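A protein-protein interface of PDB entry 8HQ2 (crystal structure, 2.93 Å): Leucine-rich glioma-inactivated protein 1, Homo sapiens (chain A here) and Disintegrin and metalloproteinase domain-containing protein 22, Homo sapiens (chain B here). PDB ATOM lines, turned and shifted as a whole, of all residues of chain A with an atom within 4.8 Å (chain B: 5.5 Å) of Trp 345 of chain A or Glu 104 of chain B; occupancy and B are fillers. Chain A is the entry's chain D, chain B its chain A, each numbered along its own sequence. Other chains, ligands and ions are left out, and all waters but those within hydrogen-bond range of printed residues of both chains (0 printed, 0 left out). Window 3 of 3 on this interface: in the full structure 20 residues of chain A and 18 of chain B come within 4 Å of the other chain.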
ATOM      1  N   LYS A 322      20.253 -24.782  -9.440  1.00  0.00           N
ATOM      2  CA  LYS A 322      19.997 -23.370  -9.712  1.00  0.00           C
ATOM      3  C   LYS A 322      19.408 -23.159 -11.104  1.00  0.00           C
ATOM      4  O   LYS A 322      18.572 -22.266 -11.292  1.00  0.00           O
ATOM      5  CB  LYS A 322      21.290 -22.566  -9.548  1.00  0.00           C
ATOM      6  CG  LYS A 322      21.239 -21.148 -10.097  1.00  0.00           C
ATOM      7  CD  LYS A 322      20.364 -20.245  -9.245  1.00  0.00           C
ATOM      8  CE  LYS A 322      21.153 -19.604  -8.126  1.00  0.00           C
ATOM      9  NZ  LYS A 322      21.208 -18.139  -8.318  1.00  0.00           N
ATOM     10  N   PHE A 325      13.919 -25.388 -12.628  1.00  0.00           N
ATOM     11  CA  PHE A 325      12.839 -24.722 -11.913  1.00  0.00           C
ATOM     12  C   PHE A 325      11.860 -25.752 -11.368  1.00  0.00           C
ATOM     13  O   PHE A 325      11.513 -26.717 -12.057  1.00  0.00           O
ATOM     14  CB  PHE A 325      12.084 -23.735 -12.820  1.00  0.00           C
ATOM     15  CG  PHE A 325      12.920 -22.583 -13.302  1.00  0.00           C
ATOM     16  CD1 PHE A 325      13.984 -22.111 -12.549  1.00  0.00           C
ATOM     17  CD2 PHE A 325      12.637 -21.965 -14.510  1.00  0.00           C
ATOM     18  CE1 PHE A 325      14.753 -21.049 -12.994  1.00  0.00           C
ATOM     19  CE2 PHE A 325      13.401 -20.901 -14.960  1.00  0.00           C
ATOM     20  CZ  PHE A 325      14.460 -20.443 -14.200  1.00  0.00           C
ATOM     21  N   HIS A 343       9.561 -20.524  -7.788  1.00  0.00           N
ATOM     22  CA  HIS A 343      10.798 -20.314  -7.033  1.00  0.00           C
ATOM     23  C   HIS A 343      12.029 -20.396  -7.937  1.00  0.00           C
ATOM     24  O   HIS A 343      12.945 -21.191  -7.722  1.00  0.00           O
ATOM     25  CB  HIS A 343      10.890 -21.313  -5.876  1.00  0.00           C
ATOM     26  CG  HIS A 343      11.558 -20.768  -4.653  1.00  0.00           C
ATOM     27  ND1 HIS A 343      11.362 -19.478  -4.205  1.00  0.00           N
ATOM     28  CD2 HIS A 343      12.404 -21.347  -3.769  1.00  0.00           C
ATOM     29  CE1 HIS A 343      12.067 -19.284  -3.105  1.00  0.00           C
ATOM     30  NE2 HIS A 343      12.711 -20.402  -2.820  1.00  0.00           N
ATOM     31  N   ALA A 344      12.022 -19.562  -8.973  1.00  0.00           N
ATOM     32  CA  ALA A 344      13.106 -19.575  -9.946  1.00  0.00           C
ATOM     33  C   ALA A 344      14.439 -19.230  -9.291  1.00  0.00           C
ATOM     34  O   ALA A 344      14.526 -18.337  -8.444  1.00  0.00           O
ATOM     35  CB  ALA A 344      12.810 -18.595 -11.080  1.00  0.00           C
ATOM     36  N   TRP A 345      15.482 -19.958  -9.696  1.00  0.00           N
ATOM     37  CA  TRP A 345      16.864 -19.709  -9.293  1.00  0.00           C
ATOM     38  C   TRP A 345      17.096 -19.942  -7.804  1.00  0.00           C
ATOM     39  O   TRP A 345      17.961 -19.306  -7.196  1.00  0.00           O
ATOM     40  CB  TRP A 345      17.318 -18.299  -9.692  1.00  0.00           C
ATOM     41  CG  TRP A 345      17.203 -18.049 -11.161  1.00  0.00           C
ATOM     42  CD1 TRP A 345      17.775 -18.776 -12.163  1.00  0.00           C
ATOM     43  CD2 TRP A 345      16.467 -17.000 -11.797  1.00  0.00           C
ATOM     44  NE1 TRP A 345      17.443 -18.245 -13.385  1.00  0.00           N
ATOM     45  CE2 TRP A 345      16.639 -17.153 -13.188  1.00  0.00           C
ATOM     46  CE3 TRP A 345      15.678 -15.946 -11.327  1.00  0.00           C
ATOM     47  CZ2 TRP A 345      16.054 -16.293 -14.111  1.00  0.00           C
ATOM     48  CZ3 TRP A 345      15.098 -15.093 -12.245  1.00  0.00           C
ATOM     49  CH2 TRP A 345      15.287 -15.270 -13.621  1.00  0.00           C
ATOM     50  N   TYR A 346      16.341 -20.859  -7.207  1.00  0.00           N
ATOM     51  CA  TYR A 346      16.605 -21.346  -5.863  1.00  0.00           C
ATOM     52  C   TYR A 346      16.818 -22.851  -5.911  1.00  0.00           C
ATOM     53  O   TYR A 346      16.409 -23.528  -6.858  1.00  0.00           O
ATOM     54  CB  TYR A 346      15.460 -21.021  -4.901  1.00  0.00           C
ATOM     55  CG  TYR A 346      15.337 -19.561  -4.534  1.00  0.00           C
ATOM     56  CD1 TYR A 346      14.662 -18.673  -5.359  1.00  0.00           C
ATOM     57  CD2 TYR A 346      15.885 -19.075  -3.355  1.00  0.00           C
ATOM     58  CE1 TYR A 346      14.545 -17.336  -5.026  1.00  0.00           C
ATOM     59  CE2 TYR A 346      15.773 -17.741  -3.013  1.00  0.00           C
ATOM     60  CZ  TYR A 346      15.102 -16.877  -3.852  1.00  0.00           C
ATOM     61  OH  TYR A 346      14.988 -15.547  -3.518  1.00  0.00           O
ATOM     62  N   ARG A 347      17.464 -23.377  -4.874  1.00  0.00           N
ATOM     63  CA  ARG A 347      17.714 -24.809  -4.761  1.00  0.00           C
ATOM     64  C   ARG A 347      16.630 -25.393  -3.866  1.00  0.00           C
ATOM     65  O   ARG A 347      16.641 -25.180  -2.652  1.00  0.00           O
ATOM     66  CB  ARG A 347      19.112 -25.067  -4.205  1.00  0.00           C
ATOM     67  CG  ARG A 347      20.206 -24.406  -5.025  1.00  0.00           C
ATOM     68  CD  ARG A 347      21.590 -24.919  -4.668  1.00  0.00           C
ATOM     69  NE  ARG A 347      22.514 -24.794  -5.794  1.00  0.00           N
ATOM     70  CZ  ARG A 347      23.206 -23.696  -6.079  1.00  0.00           C
ATOM     71  NH1 ARG A 347      23.087 -22.614  -5.321  1.00  0.00           N
ATOM     72  NH2 ARG A 347      24.021 -23.678  -7.126  1.00  0.00           N
ATOM     73  N   GLU B  71      21.713  -7.791  -9.875  1.00  0.00           N
ATOM     74  CA  GLU B  71      21.147  -9.130  -9.987  1.00  0.00           C
ATOM     75  C   GLU B  71      21.875  -9.960 -11.034  1.00  0.00           C
ATOM     76  O   GLU B  71      21.986 -11.182 -10.885  1.00  0.00           O
ATOM     77  CB  GLU B  71      19.655  -9.045 -10.317  1.00  0.00           C
ATOM     78  CG  GLU B  71      19.282  -7.943 -11.305  1.00  0.00           C
ATOM     79  CD  GLU B  71      19.053  -6.604 -10.626  1.00  0.00           C
ATOM     80  OE1 GLU B  71      18.797  -6.594  -9.403  1.00  0.00           O
ATOM     81  OE2 GLU B  71      19.132  -5.564 -11.313  1.00  0.00           O
ATOM     82  N   ASN B  72      22.372  -9.323 -12.089  1.00  0.00           N
ATOM     83  CA  ASN B  72      23.106 -10.037 -13.126  1.00  0.00           C
ATOM     84  C   ASN B  72      24.525 -10.304 -12.641  1.00  0.00           C
ATOM     85  O   ASN B  72      25.230  -9.359 -12.277  1.00  0.00           O
ATOM     86  CB  ASN B  72      23.126  -9.222 -14.418  1.00  0.00           C
ATOM     87  CG  ASN B  72      23.593 -10.027 -15.625  1.00  0.00           C
ATOM     88  OD1 ASN B  72      24.567 -10.778 -15.557  1.00  0.00           O
ATOM     89  ND2 ASN B  72      22.890  -9.870 -16.743  1.00  0.00           N
ATOM     90  N   PRO B  73      24.972 -11.562 -12.596  1.00  0.00           N
ATOM     91  CA  PRO B  73      26.341 -11.823 -12.126  1.00  0.00           C
ATOM     92  C   PRO B  73      27.410 -11.313 -13.078  1.00  0.00           C
ATOM     93  O   PRO B  73      28.508 -10.968 -12.624  1.00  0.00           O
ATOM     94  CB  PRO B  73      26.379 -13.352 -11.993  1.00  0.00           C
ATOM     95  CG  PRO B  73      25.349 -13.831 -12.963  1.00  0.00           C
ATOM     96  CD  PRO B  73      24.254 -12.801 -12.936  1.00  0.00           C
ATOM     97  N   GLN B 102      21.760 -13.212  -3.867  1.00  0.00           N
ATOM     98  CA  GLN B 102      21.642 -14.350  -4.770  1.00  0.00           C
ATOM     99  C   GLN B 102      21.403 -13.832  -6.182  1.00  0.00           C
ATOM    100  O   GLN B 102      20.452 -13.080  -6.418  1.00  0.00           O
ATOM    101  CB  GLN B 102      20.512 -15.284  -4.341  1.00  0.00           C
ATOM    102  CG  GLN B 102      20.138 -16.306  -5.400  1.00  0.00           C
ATOM    103  CD  GLN B 102      18.762 -16.888  -5.176  1.00  0.00           C
ATOM    104  OE1 GLN B 102      17.775 -16.406  -5.731  1.00  0.00           O
ATOM    105  NE2 GLN B 102      18.688 -17.934  -4.360  1.00  0.00           N
ATOM    106  N   PHE B 103      22.255 -14.236  -7.117  1.00  0.00           N
ATOM    107  CA  PHE B 103      22.102 -13.794  -8.492  1.00  0.00           C
ATOM    108  C   PHE B 103      20.908 -14.475  -9.139  1.00  0.00           C
ATOM    109  O   PHE B 103      20.679 -15.673  -8.956  1.00  0.00           O
ATOM    110  CB  PHE B 103      23.367 -14.087  -9.291  1.00  0.00           C
ATOM    111  CG  PHE B 103      24.606 -13.532  -8.670  1.00  0.00           C
ATOM    112  CD1 PHE B 103      24.763 -12.164  -8.519  1.00  0.00           C
ATOM    113  CD2 PHE B 103      25.611 -14.372  -8.229  1.00  0.00           C
ATOM    114  CE1 PHE B 103      25.900 -11.644  -7.942  1.00  0.00           C
ATOM    115  CE2 PHE B 103      26.750 -13.859  -7.648  1.00  0.00           C
ATOM    116  CZ  PHE B 103      26.892 -12.492  -7.501  1.00  0.00           C
ATOM    117  N   GLU B 104      20.152 -13.708  -9.918  1.00  0.00           N
ATOM    118  CA  GLU B 104      19.054 -14.276 -10.694  1.00  0.00           C
ATOM    119  C   GLU B 104      19.649 -14.634 -12.045  1.00  0.00           C
ATOM    120  O   GLU B 104      19.829 -13.770 -12.907  1.00  0.00           O
ATOM    121  CB  GLU B 104      17.915 -13.271 -10.826  1.00  0.00           C
ATOM    122  CG  GLU B 104      17.419 -12.709  -9.500  1.00  0.00           C
ATOM    123  CD  GLU B 104      16.280 -11.720  -9.673  1.00  0.00           C
ATOM    124  OE1 GLU B 104      15.958 -11.380 -10.832  1.00  0.00           O
ATOM    125  OE2 GLU B 104      15.706 -11.285  -8.655  1.00  0.00           O
ATOM    126  N   SER B 105      19.903 -15.923 -12.250  1.00  0.00           N
ATOM    127  CA  SER B 105      20.558 -16.433 -13.446  1.00  0.00           C
ATOM    128  C   SER B 105      20.745 -17.930 -13.259  1.00  0.00           C
ATOM    129  O   SER B 105      20.692 -18.441 -12.137  1.00  0.00           O
ATOM    130  CB  SER B 105      21.918 -15.758 -13.696  1.00  0.00           C
ATOM    131  OG  SER B 105      22.388 -16.005 -15.013  1.00  0.00           O
ATOM    132  N   SER B 106      20.994 -18.623 -14.369  1.00  0.00           N
ATOM    133  CA  SER B 106      21.374 -20.025 -14.285  1.00  0.00           C
ATOM    134  C   SER B 106      22.686 -20.201 -13.534  1.00  0.00           C
ATOM    135  O   SER B 106      22.907 -21.241 -12.904  1.00  0.00           O
ATOM    136  CB  SER B 106      21.493 -20.616 -15.689  1.00  0.00           C
ATOM    137  OG  SER B 106      22.277 -21.795 -15.665  1.00  0.00           O
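The backbone carbonyl oxygen (O) of Phe 103 of chain B lies within hydrogen-bond range of the side-chain amino group (NZ) of Lys 322 of chain A, at 2.6 Å. The side-chain amide nitrogen (NE2) of Gln 102 of chain B lies within hydrogen-bond range of the backbone carbonyl oxygen (O) of Trp 345 of chain A, at 3.2 Å. NE1 of Trp 345 of chain A sits close to O of Ser 105 of chain B (3.5 Å).
The backbone NH (N) of Glu 104 of chain B is in hydrogen-bond range of the backbone carbonyl oxygen (O) of Glu 71 of chain B, 3.3 Å away.
Among the printed residues, merely in contact across the chains: Tyr 346 of chain A with Gln 102 of chain B (3.2 Å), Lys 322 of chain A with Ser 106 of chain B (3.3 Å), Lys 322 of chain A with Ser 105 of chain B (3.4 Å), Trp 345 of chain A with Glu 104 of chain B (3.5 Å), Lys 322 of chain A with Gln 102 of chain B (3.6 Å) and Trp 345 of chain A with Ser 106 of chain B (3.7 Å).
Printed residues of chain B within 4 Å of Lys 322 of chain A: Gln 102, Phe 103, Ser 105 and Ser 106. Of chain B, only Gln 102 (3.2 Å), Glu 104 (3.5 Å), Ser 105 (2.9 Å) and Ser 106 (3.7 Å) come within 4 Å of Trp 345 of chain A. Printed residues of chain B within 4 Å of Tyr 346 of chain A: Gln 102 (3.2 Å). Printed residues of chain A within 4 Å of Phe 103 of chain B: Lys 322 (2.6 Å). Of chain A, only Trp 345 comes within 4 Å of Glu 104 of chain B. Of the printed residues of chain A, Ser 105 of chain B touches Lys 322 and Trp 345. Of the printed residues of chain A, Ser 106 of chain B touches Lys 322 and Trp 345. The nearest residue of chain B that does not touch Trp 345 of chain A is Phe 103 of chain B (4.3 Å). The nearest printed residue of chain A that does not touch Glu 104 of chain B is Lys 322 of chain A (4.8 Å). The nearest printed residue of chain A that does not touch Gln 102 of chain B is Ala 344 of chain A (4.7 Å).
Printed residues of chain A that touch a printed residue of chain B: Lys 322, Trp 345 and Tyr 346. Hydrophobic or aromatic side chains of chain A that line the printed part of chain B: Trp 345 and Tyr 346. Among the printed residues, 9 pairs touch across the chains. Among the printed residues, no Asp or Glu carboxylate lies within 4 Å of a Lys or Arg side-chain nitrogen of the other chain.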
